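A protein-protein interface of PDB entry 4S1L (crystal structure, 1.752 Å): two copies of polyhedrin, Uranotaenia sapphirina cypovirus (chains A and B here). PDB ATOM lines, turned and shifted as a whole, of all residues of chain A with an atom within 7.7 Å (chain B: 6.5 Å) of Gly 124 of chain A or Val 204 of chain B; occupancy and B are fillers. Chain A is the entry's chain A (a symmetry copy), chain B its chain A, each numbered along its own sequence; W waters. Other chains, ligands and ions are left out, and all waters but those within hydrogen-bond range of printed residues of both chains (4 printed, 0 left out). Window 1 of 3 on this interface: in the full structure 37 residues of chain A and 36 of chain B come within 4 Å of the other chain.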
ATOM      1  N   LYS A  52     -28.452  37.790 -36.168  1.00  0.00           N
ATOM      2  CA  LYS A  52     -28.188  36.489 -35.564  1.00  0.00           C
ATOM      3  C   LYS A  52     -26.745  36.511 -35.073  1.00  0.00           C
ATOM      4  O   LYS A  52     -25.816  36.339 -35.850  1.00  0.00           O
ATOM      5  CB  LYS A  52     -28.423  35.368 -36.569  1.00  0.00           C
ATOM      6  CG  LYS A  52     -29.896  35.249 -36.931  1.00  0.00           C
ATOM      7  CD  LYS A  52     -30.210  34.259 -38.008  1.00  0.00           C
ATOM      8  CE  LYS A  52     -31.718  34.289 -38.265  1.00  0.00           C
ATOM      9  NZ  LYS A  52     -32.220  33.255 -39.214  1.00  0.00           N
ATOM     10  N   GLY A  53     -26.558  36.822 -33.797  1.00  0.00           N
ATOM     11  CA  GLY A  53     -25.228  36.917 -33.208  1.00  0.00           C
ATOM     12  C   GLY A  53     -24.899  35.623 -32.503  1.00  0.00           C
ATOM     13  O   GLY A  53     -25.327  35.397 -31.366  1.00  0.00           O
ATOM     14  N   VAL A  54     -24.143  34.760 -33.189  1.00  0.00           N
ATOM     15  CA  VAL A  54     -23.854  33.417 -32.704  1.00  0.00           C
ATOM     16  C   VAL A  54     -22.363  33.266 -32.465  1.00  0.00           C
ATOM     17  O   VAL A  54     -21.576  33.438 -33.390  1.00  0.00           O
ATOM     18  CB  VAL A  54     -24.329  32.372 -33.722  1.00  0.00           C
ATOM     19  CG1 VAL A  54     -24.083  30.952 -33.203  1.00  0.00           C
ATOM     20  CG2 VAL A  54     -25.819  32.610 -34.053  1.00  0.00           C
ATOM     21  N   ILE A  55     -21.984  32.986 -31.217  1.00  0.00           N
ATOM     22  CA  ILE A  55     -20.581  32.896 -30.836  1.00  0.00           C
ATOM     23  C   ILE A  55     -20.318  31.580 -30.118  1.00  0.00           C
ATOM     24  O   ILE A  55     -20.993  31.234 -29.139  1.00  0.00           O
ATOM     25  CB  ILE A  55     -20.162  34.079 -29.942  1.00  0.00           C
ATOM     26  CG1 ILE A  55     -20.526  35.396 -30.621  1.00  0.00           C
ATOM     27  CG2 ILE A  55     -18.638  34.027 -29.652  1.00  0.00           C
ATOM     28  CD1 ILE A  55     -20.160  36.608 -29.814  1.00  0.00           C
ATOM     29  N   LYS A  56     -19.344  30.846 -30.648  1.00  0.00           N
ATOM     30  CA  LYS A  56     -18.873  29.612 -30.058  1.00  0.00           C
ATOM     31  C   LYS A  56     -18.099  29.903 -28.792  1.00  0.00           C
ATOM     32  O   LYS A  56     -17.542  30.990 -28.626  1.00  0.00           O
ATOM     33  CB  LYS A  56     -17.980  28.853 -31.048  1.00  0.00           C
ATOM     34  CG  LYS A  56     -18.733  28.362 -32.248  1.00  0.00           C
ATOM     35  CD  LYS A  56     -17.805  27.911 -33.390  1.00  0.00           C
ATOM     36  CE  LYS A  56     -16.945  26.740 -33.032  1.00  0.00           C
ATOM     37  NZ  LYS A  56     -16.183  26.273 -34.243  1.00  0.00           N
ATOM     38  N   SER A  57     -18.055  28.927 -27.888  1.00  0.00           N
ATOM     39  CA  SER A  57     -17.334  29.096 -26.641  1.00  0.00           C
ATOM     40  C   SER A  57     -15.823  29.274 -26.903  1.00  0.00           C
ATOM     41  O   SER A  57     -15.144  30.011 -26.195  1.00  0.00           O
ATOM     42  CB  SER A  57     -17.579  27.899 -25.715  1.00  0.00           C
ATOM     43  OG  SER A  57     -17.205  26.678 -26.349  1.00  0.00           O
ATOM     44  N   ASP A 118     -29.444  34.629 -25.244  1.00  0.00           N
ATOM     45  CA  ASP A 118     -29.404  33.312 -24.631  1.00  0.00           C
ATOM     46  C   ASP A 118     -27.940  32.929 -24.348  1.00  0.00           C
ATOM     47  O   ASP A 118     -27.118  32.823 -25.260  1.00  0.00           O
ATOM     48  CB  ASP A 118     -30.105  32.334 -25.571  1.00  0.00           C
ATOM     49  CG  ASP A 118     -30.337  30.962 -24.965  1.00  0.00           C
ATOM     50  OD1 ASP A 118     -30.202  30.800 -23.739  1.00  0.00           O
ATOM     51  OD2 ASP A 118     -30.678  30.056 -25.747  1.00  0.00           O
ATOM     52  N   ARG A 120     -25.640  30.147 -23.384  1.00  0.00           N
ATOM     53  CA  ARG A 120     -25.779  28.701 -23.526  1.00  0.00           C
ATOM     54  C   ARG A 120     -24.518  28.035 -22.989  1.00  0.00           C
ATOM     55  O   ARG A 120     -23.568  28.713 -22.650  1.00  0.00           O
ATOM     56  CB  ARG A 120     -26.013  28.317 -24.996  1.00  0.00           C
ATOM     57  CG  ARG A 120     -27.264  28.988 -25.597  1.00  0.00           C
ATOM     58  CD  ARG A 120     -27.424  28.713 -27.064  1.00  0.00           C
ATOM     59  NE  ARG A 120     -27.757  27.314 -27.313  1.00  0.00           N
ATOM     60  CZ  ARG A 120     -28.982  26.800 -27.252  1.00  0.00           C
ATOM     61  NH1 ARG A 120     -30.030  27.546 -26.920  1.00  0.00           N
ATOM     62  NH2 ARG A 120     -29.158  25.515 -27.506  1.00  0.00           N
ATOM     63  N   GLY A 121     -24.518  26.710 -22.927  1.00  0.00           N
ATOM     64  CA  GLY A 121     -23.425  25.978 -22.335  1.00  0.00           C
ATOM     65  C   GLY A 121     -22.187  25.943 -23.198  1.00  0.00           C
ATOM     66  O   GLY A 121     -22.169  26.444 -24.331  1.00  0.00           O
ATOM     67  N   PRO A 122     -21.122  25.334 -22.662  1.00  0.00           N
ATOM     68  CA  PRO A 122     -19.796  25.360 -23.311  1.00  0.00           C
ATOM     69  C   PRO A 122     -19.720  24.614 -24.640  1.00  0.00           C
ATOM     70  O   PRO A 122     -18.739  24.805 -25.374  1.00  0.00           O
ATOM     71  CB  PRO A 122     -18.876  24.707 -22.262  1.00  0.00           C
ATOM     72  CG  PRO A 122     -19.775  24.004 -21.280  1.00  0.00           C
ATOM     73  CD  PRO A 122     -21.113  24.697 -21.333  1.00  0.00           C
ATOM     74  N   THR A 123     -20.696  23.765 -24.942  1.00  0.00           N
ATOM     75  CA  THR A 123     -20.721  23.083 -26.227  1.00  0.00           C
ATOM     76  C   THR A 123     -21.985  23.434 -27.004  1.00  0.00           C
ATOM     77  O   THR A 123     -22.312  22.777 -27.993  1.00  0.00           O
ATOM     78  CB  THR A 123     -20.618  21.548 -26.073  1.00  0.00           C
ATOM     79  OG1 THR A 123     -21.727  21.041 -25.310  1.00  0.00           O
ATOM     80  CG2 THR A 123     -19.314  21.192 -25.379  1.00  0.00           C
ATOM     81  N   GLY A 124     -22.678  24.485 -26.563  1.00  0.00           N
ATOM     82  CA  GLY A 124     -23.787  25.040 -27.326  1.00  0.00           C
ATOM     83  C   GLY A 124     -25.169  24.563 -26.925  1.00  0.00           C
ATOM     84  O   GLY A 124     -26.148  24.935 -27.565  1.00  0.00           O
ATOM     85  N   LEU A 125     -25.252  23.736 -25.884  1.00  0.00           N
ATOM     86  CA  LEU A 125     -26.555  23.255 -25.401  1.00  0.00           C
ATOM     87  C   LEU A 125     -27.230  24.288 -24.497  1.00  0.00           C
ATOM     88  O   LEU A 125     -26.555  25.104 -23.876  1.00  0.00           O
ATOM     89  CB  LEU A 125     -26.397  21.943 -24.624  1.00  0.00           C
ATOM     90  CG  LEU A 125     -25.709  20.770 -25.318  1.00  0.00           C
ATOM     91  CD1 LEU A 125     -25.838  19.481 -24.480  1.00  0.00           C
ATOM     92  CD2 LEU A 125     -26.315  20.580 -26.673  1.00  0.00           C
ATOM     93  N   SER A 126     -28.559  24.241 -24.399  1.00  0.00           N
ATOM     94  CA  SER A 126     -29.258  25.048 -23.394  1.00  0.00           C
ATOM     95  C   SER A 126     -28.622  24.860 -22.018  1.00  0.00           C
ATOM     96  O   SER A 126     -28.350  23.727 -21.601  1.00  0.00           O
ATOM     97  CB  SER A 126     -30.741  24.672 -23.309  1.00  0.00           C
ATOM     98  OG  SER A 126     -31.392  24.839 -24.561  1.00  0.00           O
ATOM     99  N   MET A 127     -28.397  25.969 -21.323  1.00  0.00           N
ATOM    100  CA  MET A 127     -27.685  25.927 -20.048  1.00  0.00           C
ATOM    101  C   MET A 127     -28.582  25.443 -18.918  1.00  0.00           C
ATOM    102  O   MET A 127     -29.724  25.869 -18.777  1.00  0.00           O
ATOM    103  CB  MET A 127     -27.112  27.299 -19.693  1.00  0.00           C
ATOM    104  CG  MET A 127     -26.165  27.214 -18.483  1.00  0.00           C
ATOM    105  SD  MET A 127     -25.574  28.832 -17.966  1.00  0.00           S
ATOM    106  CE  MET A 127     -24.368  29.091 -19.240  1.00  0.00           C
ATOM    107  N   GLU A 131     -26.622  19.396 -18.480  1.00  0.00           N
ATOM    108  CA  GLU A 131     -26.887  19.609 -19.900  1.00  0.00           C
ATOM    109  C   GLU A 131     -27.019  18.275 -20.614  1.00  0.00           C
ATOM    110  O   GLU A 131     -26.264  17.345 -20.337  1.00  0.00           O
ATOM    111  CB  GLU A 131     -25.773  20.461 -20.515  1.00  0.00           C
ATOM    112  CG  GLU A 131     -25.808  21.882 -19.957  1.00  0.00           C
ATOM    113  CD  GLU A 131     -24.702  22.789 -20.476  1.00  0.00           C
ATOM    114  OE1 GLU A 131     -23.958  22.390 -21.391  1.00  0.00           O
ATOM    115  OE2 GLU A 131     -24.615  23.926 -19.968  1.00  0.00           O
ATOM    116  N   TYR A 133     -28.772  16.305 -24.507  1.00  0.00           N
ATOM    117  CA  TYR A 133     -29.376  16.554 -25.829  1.00  0.00           C
ATOM    118  C   TYR A 133     -30.907  16.558 -25.806  1.00  0.00           C
ATOM    119  O   TYR A 133     -31.540  17.290 -26.554  1.00  0.00           O
ATOM    120  CB  TYR A 133     -28.879  15.518 -26.844  1.00  0.00           C
ATOM    121  CG  TYR A 133     -27.499  15.801 -27.383  1.00  0.00           C
ATOM    122  CD1 TYR A 133     -27.149  17.071 -27.817  1.00  0.00           C
ATOM    123  CD2 TYR A 133     -26.544  14.802 -27.464  1.00  0.00           C
ATOM    124  CE1 TYR A 133     -25.880  17.343 -28.318  1.00  0.00           C
ATOM    125  CE2 TYR A 133     -25.273  15.070 -27.949  1.00  0.00           C
ATOM    126  CZ  TYR A 133     -24.959  16.346 -28.386  1.00  0.00           C
ATOM    127  OH  TYR A 133     -23.685  16.609 -28.869  1.00  0.00           O
ATOM    128  N   ASP A 136     -32.768  20.404 -25.008  1.00  0.00           N
ATOM    129  CA  ASP A 136     -31.994  21.401 -25.728  1.00  0.00           C
ATOM    130  C   ASP A 136     -32.968  22.148 -26.649  1.00  0.00           C
ATOM    131  O   ASP A 136     -33.674  21.528 -27.463  1.00  0.00           O
ATOM    132  CB  ASP A 136     -30.849  20.729 -26.506  1.00  0.00           C
ATOM    133  CG  ASP A 136     -29.965  21.739 -27.254  1.00  0.00           C
ATOM    134  OD1 ASP A 136     -29.649  22.816 -26.693  1.00  0.00           O
ATOM    135  OD2 ASP A 136     -29.600  21.451 -28.420  1.00  0.00           O
ATOM    136  N   ARG A 137     -33.033  23.468 -26.500  1.00  0.00           N
ATOM    137  CA  ARG A 137     -34.060  24.262 -27.174  1.00  0.00           C
ATOM    138  C   ARG A 137     -33.545  25.675 -27.399  1.00  0.00           C
ATOM    139  O   ARG A 137     -32.450  26.022 -26.929  1.00  0.00           O
ATOM    140  CB  ARG A 137     -35.353  24.252 -26.357  1.00  0.00           C
ATOM    141  CG  ARG A 137     -35.239  24.668 -24.884  1.00  0.00           C
ATOM    142  CD  ARG A 137     -35.302  26.188 -24.643  1.00  0.00           C
ATOM    143  NE  ARG A 137     -36.513  26.783 -25.197  1.00  0.00           N
ATOM    144  CZ  ARG A 137     -37.710  26.761 -24.621  1.00  0.00           C
ATOM    145  NH1 ARG A 137     -37.894  26.163 -23.452  1.00  0.00           N
ATOM    146  NH2 ARG A 137     -38.739  27.322 -25.229  1.00  0.00           N
ATOM    147  N   ILE A 138     -34.303  26.485 -28.137  1.00  0.00           N
ATOM    148  CA  ILE A 138     -33.918  27.885 -28.335  1.00  0.00           C
ATOM    149  C   ILE A 138     -34.982  28.808 -27.739  1.00  0.00           C
ATOM    150  O   ILE A 138     -36.080  28.373 -27.405  1.00  0.00           O
ATOM    151  CB  ILE A 138     -33.682  28.230 -29.818  1.00  0.00           C
ATOM    152  CG1 ILE A 138     -34.993  28.248 -30.630  1.00  0.00           C
ATOM    153  CG2 ILE A 138     -32.654  27.251 -30.431  1.00  0.00           C
ATOM    154  CD1 ILE A 138     -34.824  28.774 -32.054  1.00  0.00           C
ATOM    155  N   VAL A 172     -18.946  29.795 -21.684  1.00  0.00           N
ATOM    156  CA  VAL A 172     -20.309  29.824 -22.203  1.00  0.00           C
ATOM    157  C   VAL A 172     -20.251  30.062 -23.712  1.00  0.00           C
ATOM    158  O   VAL A 172     -19.202  30.442 -24.250  1.00  0.00           O
ATOM    159  CB  VAL A 172     -21.152  30.934 -21.534  1.00  0.00           C
ATOM    160  CG1 VAL A 172     -21.237  30.734 -20.034  1.00  0.00           C
ATOM    161  CG2 VAL A 172     -20.575  32.298 -21.845  1.00  0.00           C
ATOM    162  N   SER A 173     -21.379  29.842 -24.377  1.00  0.00           N
ATOM    163  CA  SER A 173     -21.560  30.235 -25.776  1.00  0.00           C
ATOM    164  C   SER A 173     -22.758  31.164 -25.819  1.00  0.00           C
ATOM    165  O   SER A 173     -23.473  31.285 -24.839  1.00  0.00           O
ATOM    166  CB  SER A 173     -21.754  29.016 -26.684  1.00  0.00           C
ATOM    167  OG  SER A 173     -22.820  28.201 -26.215  1.00  0.00           O
ATOM    168  N   ILE A 174     -22.988  31.796 -26.965  1.00  0.00           N
ATOM    169  CA  ILE A 174     -23.946  32.891 -27.053  1.00  0.00           C
ATOM    170  C   ILE A 174     -24.812  32.766 -28.286  1.00  0.00           C
ATOM    171  O   ILE A 174     -24.289  32.527 -29.390  1.00  0.00           O
ATOM    172  CB  ILE A 174     -23.237  34.253 -27.114  1.00  0.00           C
ATOM    173  CG1 ILE A 174     -22.494  34.531 -25.806  1.00  0.00           C
ATOM    174  CG2 ILE A 174     -24.236  35.364 -27.367  1.00  0.00           C
ATOM    175  CD1 ILE A 174     -21.667  35.781 -25.867  1.00  0.00           C
ATOM    176  N   ALA A 175     -26.117  32.972 -28.102  1.00  0.00           N
ATOM    177  CA  ALA A 175     -27.045  33.126 -29.232  1.00  0.00           C
ATOM    178  C   ALA A 175     -27.922  34.341 -29.008  1.00  0.00           C
ATOM    179  O   ALA A 175     -28.712  34.371 -28.071  1.00  0.00           O
ATOM    180  CB  ALA A 175     -27.910  31.870 -29.414  1.00  0.00           C
ATOM    181  N   ILE A 177     -30.702  36.894 -30.846  1.00  0.00           N
ATOM    182  CA  ILE A 177     -31.622  37.046 -31.966  1.00  0.00           C
ATOM    183  C   ILE A 177     -32.277  38.420 -31.808  1.00  0.00           C
ATOM    184  O   ILE A 177     -32.952  38.653 -30.804  1.00  0.00           O
ATOM    185  CB  ILE A 177     -32.696  35.938 -32.004  1.00  0.00           C
ATOM    186  CG1 ILE A 177     -32.040  34.557 -32.073  1.00  0.00           C
ATOM    187  CG2 ILE A 177     -33.620  36.140 -33.201  1.00  0.00           C
ATOM    188  CD1 ILE A 177     -32.999  33.378 -31.808  1.00  0.00           C
ATOM    189  N   ASN B  26     -34.727  21.669 -30.206  1.00  0.00           N
ATOM    190  CA  ASN B  26     -33.772  21.334 -31.250  1.00  0.00           C
ATOM    191  C   ASN B  26     -33.821  19.868 -31.699  1.00  0.00           C
ATOM    192  O   ASN B  26     -33.953  18.940 -30.877  1.00  0.00           O
ATOM    193  CB  ASN B  26     -32.355  21.654 -30.772  1.00  0.00           C
ATOM    194  CG  ASN B  26     -32.040  23.136 -30.835  1.00  0.00           C
ATOM    195  OD1 ASN B  26     -32.548  23.848 -31.694  1.00  0.00           O
ATOM    196  ND2 ASN B  26     -31.183  23.604 -29.939  1.00  0.00           N
ATOM    197  N   HIS B  44     -20.917  19.133 -34.094  1.00  0.00           N
ATOM    198  CA  HIS B  44     -22.311  19.155 -33.605  1.00  0.00           C
ATOM    199  C   HIS B  44     -23.062  20.350 -34.147  1.00  0.00           C
ATOM    200  O   HIS B  44     -22.552  21.469 -34.091  1.00  0.00           O
ATOM    201  CB  HIS B  44     -22.380  19.171 -32.064  1.00  0.00           C
ATOM    202  CG  HIS B  44     -23.760  19.413 -31.550  1.00  0.00           C
ATOM    203  ND1 HIS B  44     -24.179  20.648 -31.099  1.00  0.00           N
ATOM    204  CD2 HIS B  44     -24.837  18.597 -31.475  1.00  0.00           C
ATOM    205  CE1 HIS B  44     -25.454  20.575 -30.755  1.00  0.00           C
ATOM    206  NE2 HIS B  44     -25.880  19.344 -30.977  1.00  0.00           N
ATOM    207  N   PHE B  45     -24.279  20.100 -34.655  1.00  0.00           N
ATOM    208  CA  PHE B  45     -25.179  21.140 -35.185  1.00  0.00           C
ATOM    209  C   PHE B  45     -26.554  20.905 -34.592  1.00  0.00           C
ATOM    210  O   PHE B  45     -26.927  19.764 -34.318  1.00  0.00           O
ATOM    211  CB  PHE B  45     -25.333  21.102 -36.707  1.00  0.00           C
ATOM    212  CG  PHE B  45     -24.053  21.164 -37.460  1.00  0.00           C
ATOM    213  CD1 PHE B  45     -23.310  20.013 -37.669  1.00  0.00           C
ATOM    214  CD2 PHE B  45     -23.594  22.372 -37.977  1.00  0.00           C
ATOM    215  CE1 PHE B  45     -22.104  20.064 -38.372  1.00  0.00           C
ATOM    216  CE2 PHE B  45     -22.394  22.432 -38.684  1.00  0.00           C
ATOM    217  CZ  PHE B  45     -21.653  21.272 -38.873  1.00  0.00           C
ATOM    218  N   ALA B  46     -27.320  21.968 -34.423  1.00  0.00           N
ATOM    219  CA  ALA B  46     -28.681  21.834 -33.921  1.00  0.00           C
ATOM    220  C   ALA B  46     -29.563  22.966 -34.384  1.00  0.00           C
ATOM    221  O   ALA B  46     -29.109  24.102 -34.540  1.00  0.00           O
ATOM    222  CB  ALA B  46     -28.685  21.780 -32.383  1.00  0.00           C
ATOM    223  N   ASN B  47     -30.845  22.649 -34.550  1.00  0.00           N
ATOM    224  CA  ASN B  47     -31.860  23.652 -34.873  1.00  0.00           C
ATOM    225  C   ASN B  47     -33.234  23.043 -34.694  1.00  0.00           C
ATOM    226  O   ASN B  47     -33.364  21.824 -34.784  1.00  0.00           O
ATOM    227  CB  ASN B  47     -31.729  24.161 -36.309  1.00  0.00           C
ATOM    228  CG  ASN B  47     -32.510  25.445 -36.537  1.00  0.00           C
ATOM    229  OD1 ASN B  47     -33.628  25.444 -37.095  1.00  0.00           O
ATOM    230  ND2 ASN B  47     -31.941  26.557 -36.067  1.00  0.00           N
ATOM    231  N   PRO B  48     -34.264  23.877 -34.465  1.00  0.00           N
ATOM    232  CA  PRO B  48     -35.581  23.246 -34.343  1.00  0.00           C
ATOM    233  C   PRO B  48     -36.276  23.018 -35.654  1.00  0.00           C
ATOM    234  O   PRO B  48     -37.211  22.216 -35.673  1.00  0.00           O
ATOM    235  CB  PRO B  48     -36.391  24.257 -33.519  1.00  0.00           C
ATOM    236  CG  PRO B  48     -35.368  25.125 -32.846  1.00  0.00           C
ATOM    237  CD  PRO B  48     -34.263  25.229 -33.854  1.00  0.00           C
ATOM    238  N   GLY B 200     -35.575  31.905 -36.094  1.00  0.00           N
ATOM    239  CA  GLY B 200     -34.942  30.814 -35.368  1.00  0.00           C
ATOM    240  C   GLY B 200     -33.925  29.982 -36.161  1.00  0.00           C
ATOM    241  O   GLY B 200     -33.134  29.228 -35.581  1.00  0.00           O
ATOM    242  N   LEU B 201     -33.951  30.098 -37.487  1.00  0.00           N
ATOM    243  CA  LEU B 201     -32.963  29.407 -38.322  1.00  0.00           C
ATOM    244  C   LEU B 201     -31.552  29.871 -38.047  1.00  0.00           C
ATOM    245  O   LEU B 201     -31.295  31.062 -37.922  1.00  0.00           O
ATOM    246  CB  LEU B 201     -33.261  29.620 -39.795  1.00  0.00           C
ATOM    247  CG  LEU B 201     -34.621  29.141 -40.305  1.00  0.00           C
ATOM    248  CD1 LEU B 201     -34.848  29.577 -41.746  1.00  0.00           C
ATOM    249  CD2 LEU B 201     -34.678  27.647 -40.207  1.00  0.00           C
ATOM    250  N   ASP B 202     -30.631  28.913 -37.967  1.00  0.00           N
ATOM    251  CA  ASP B 202     -29.203  29.210 -37.926  1.00  0.00           C
ATOM    252  C   ASP B 202     -28.801  30.024 -36.684  1.00  0.00           C
ATOM    253  O   ASP B 202     -27.984  30.935 -36.792  1.00  0.00           O
ATOM    254  CB  ASP B 202     -28.761  29.993 -39.187  1.00  0.00           C
ATOM    255  CG  ASP B 202     -29.183  29.332 -40.474  1.00  0.00           C
ATOM    256  OD1 ASP B 202     -29.011  28.104 -40.605  1.00  0.00           O
ATOM    257  OD2 ASP B 202     -29.698  30.054 -41.353  1.00  0.00           O
ATOM    258  N   THR B 203     -29.352  29.691 -35.522  1.00  0.00           N
ATOM    259  CA  THR B 203     -29.111  30.491 -34.324  1.00  0.00           C
ATOM    260  C   THR B 203     -28.396  29.742 -33.187  1.00  0.00           C
ATOM    261  O   THR B 203     -28.232  30.309 -32.118  1.00  0.00           O
ATOM    262  CB  THR B 203     -30.440  31.057 -33.748  1.00  0.00           C
ATOM    263  OG1 THR B 203     -31.330  29.988 -33.451  1.00  0.00           O
ATOM    264  CG2 THR B 203     -31.133  32.011 -34.726  1.00  0.00           C
ATOM    265  N   VAL B 204     -27.964  28.502 -33.424  1.00  0.00           N
ATOM    266  CA  VAL B 204     -27.324  27.686 -32.391  1.00  0.00           C
ATOM    267  C   VAL B 204     -25.832  27.526 -32.682  1.00  0.00           C
ATOM    268  O   VAL B 204     -25.464  27.123 -33.783  1.00  0.00           O
ATOM    269  CB  VAL B 204     -27.969  26.289 -32.299  1.00  0.00           C
ATOM    270  CG1 VAL B 204     -27.400  25.513 -31.136  1.00  0.00           C
ATOM    271  CG2 VAL B 204     -29.475  26.420 -32.171  1.00  0.00           C
ATOM    272  N   PRO B 205     -24.971  27.819 -31.698  1.00  0.00           N
ATOM    273  CA  PRO B 205     -23.537  27.653 -31.958  1.00  0.00           C
ATOM    274  C   PRO B 205     -23.154  26.213 -32.277  1.00  0.00           C
ATOM    275  O   PRO B 205     -23.661  25.305 -31.645  1.00  0.00           O
ATOM    276  CB  PRO B 205     -22.880  28.086 -30.642  1.00  0.00           C
ATOM    277  CG  PRO B 205     -23.902  28.804 -29.869  1.00  0.00           C
ATOM    278  CD  PRO B 205     -25.231  28.277 -30.319  1.00  0.00           C
ATOM    279  N   GLU B 206     -22.271  26.046 -33.262  1.00  0.00           N
ATOM    280  CA  GLU B 206     -21.652  24.766 -33.614  1.00  0.00           C
ATOM    281  C   GLU B 206     -20.599  24.395 -32.583  1.00  0.00           C
ATOM    282  O   GLU B 206     -20.177  25.240 -31.793  1.00  0.00           O
ATOM    283  CB  GLU B 206     -21.024  24.864 -35.014  1.00  0.00           C
ATOM    284  CG  GLU B 206     -20.453  23.554 -35.619  1.00  0.00           C
ATOM    285  CD  GLU B 206     -18.955  23.310 -35.350  1.00  0.00           C
ATOM    286  OE1 GLU B 206     -18.212  24.262 -35.025  1.00  0.00           O
ATOM    287  OE2 GLU B 206     -18.524  22.140 -35.493  1.00  0.00           O
ATOM    288  N   CYS B 207     -20.188  23.130 -32.567  1.00  0.00           N
ATOM    289  CA  CYS B 207     -19.047  22.724 -31.746  1.00  0.00           C
ATOM    290  C   CYS B 207     -18.258  21.589 -32.391  1.00  0.00           C
ATOM    291  O   CYS B 207     -18.818  20.545 -32.751  1.00  0.00           O
ATOM    292  CB  CYS B 207     -19.503  22.293 -30.356  1.00  0.00           C
ATOM    293  SG  CYS B 207     -18.140  21.877 -29.192  1.00  0.00           S
HETATM  294  O   HOH W   1     -19.469  26.243 -28.885  1.00  0.00           O
HETATM  295  O   HOH W   2     -33.586  17.829 -28.432  1.00  0.00           O
HETATM  296  O   HOH W   3     -22.968  22.952 -30.603  1.00  0.00           O
HETATM  297  O   HOH W   4     -31.016  32.906 -41.475  1.00  0.00           O
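Gly 124 of chain A touches one residue of chain B.
Of the printed residues of chain B, Thr 123 of chain A touches Cys 207 (3.7 Å).
Printed residues of chain A within 4 Å of His 44 of chain B: Tyr 133.
Printed residues of chain A within 4 Å of Asp 202 of chain B: Val 54 (3.9 Å).
Of the printed residues of chain B, Tyr 133 of chain A touches His 44 (3.3 Å).
The nearest printed residue of chain B that does not touch Arg 120 of chain A is Val 204 of chain B (4.03 Å).
The side-chain amide nitrogen of Asn 47 of chain B sits at hydrogen-bond distance from the backbone carbonyl oxygen of Gly 200 of chain B.
OG1 of Thr 203 of chain B sits at hydrogen-bond distance from O of Gly 200 of chain B (2.9 Å).
The backbone NH of Ile 55 of chain A sits at hydrogen-bond distance from the backbone carbonyl oxygen of Ile 174 of chain A.
N of Asp 118 of chain A sits at hydrogen-bond distance from O of Ala 175 of chain A (2.9 Å).
NH2 of Arg 120 of chain A is in salt-bridge range of OD1 of Asp 136 of chain A.
The backbone carbonyl oxygen (O) of Arg 137 of chain A lies within hydrogen-bond range of the side-chain hydroxyl (OG) of Ser 126 of chain A (2.9 Å).
Val 54 of chain A touches Asp 202 of chain B.
Val 54 of chain A touches Val 204 of chain B.
Ile 55 of chain A touches Pro 205 of chain B.
Asn 26 of chain B touches Arg 120 of chain A (ND2 to NH2, 3.7 Å).
Tyr 133 of chain A touches His 44 of chain B (CE1 to NE2, 3.3 Å).
Asn 26 of chain B touches Ile 138 of chain A (OD1 to CG2, 3.6 Å).
Ile 138 of chain A touches Pro 48 of chain B.
CD1 of Ile 138 of chain A touches OG1 of Thr 203 of chain B, at 3.95 Å.
Ser 173 of chain A touches Pro 205 of chain B (CB to CG, 3.8 Å).
CG2 of Thr 203 of chain B touches CD1 of Ile 177 of chain A, 3.7 Å away.
No position is printed for both chains.
Of the 23 pairs that touch across the chains among the printed residues, none has its exchanged pair printed and touching as well.
Water W4 bridges the side-chain amino group (NZ) of Lys 52 of chain A (2.6 Å) and the side-chain carboxylate (OD2) of Asp 202 of chain B (3.1 Å).
Water W3 lies within hydrogen-bond range of ND1 of His 44 of chain B (2.6 Å), O of Pro 205 of chain B (2.7 Å), O of Thr 123 of chain A (2.7 Å) and N of Cys 207 of chain B (3.4 Å).
Water W2 lies within hydrogen-bond range of the backbone carbonyl oxygen of Asn 26 of chain B (2.7 Å) and the backbone carbonyl oxygen of Tyr 133 of chain A (2.8 Å).
Water W1 lies within hydrogen-bond range of the backbone carbonyl oxygen of Glu 206 of chain B and the backbone NH of Ser 57 of chain A.
The backbone carbonyl oxygen (O) of Asp 136 of chain A is in hydrogen-bond range of the backbone NH (N) of Asn 26 of chain B (2.9 Å).
O of Leu 201 of chain B lies within hydrogen-bond range of NZ of Lys 52 of chain A, at 2.7 Å.
The side-chain carboxylate of Glu 206 of chain B is in salt-bridge range of the side-chain amino group of Lys 56 of chain A (3.0 Å).
Printed residues of chain A that touch a printed residue of chain B: Lys 52, Val 54, Ile 55, Lys 56, Arg 120, Thr 123, Gly 124, Tyr 133, Asp 136, Arg 137, Ile 138, Ser 173, Ile 174, Ala 175 and Ile 177.
Of the 14 printed residues of chain B, 11 touch a printed residue of chain A.
Hydrophobic or aromatic side chains of chain B within 4 Å of the printed part of chain A: His 44, Pro 48, Leu 201, Val 204 and Pro 205.
Among the printed residues, Asp or Glu carboxylates within 4 Å of a Lys or Arg side-chain nitrogen of the other chain: Lys 56 of chain A with Glu 206 of chain B.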
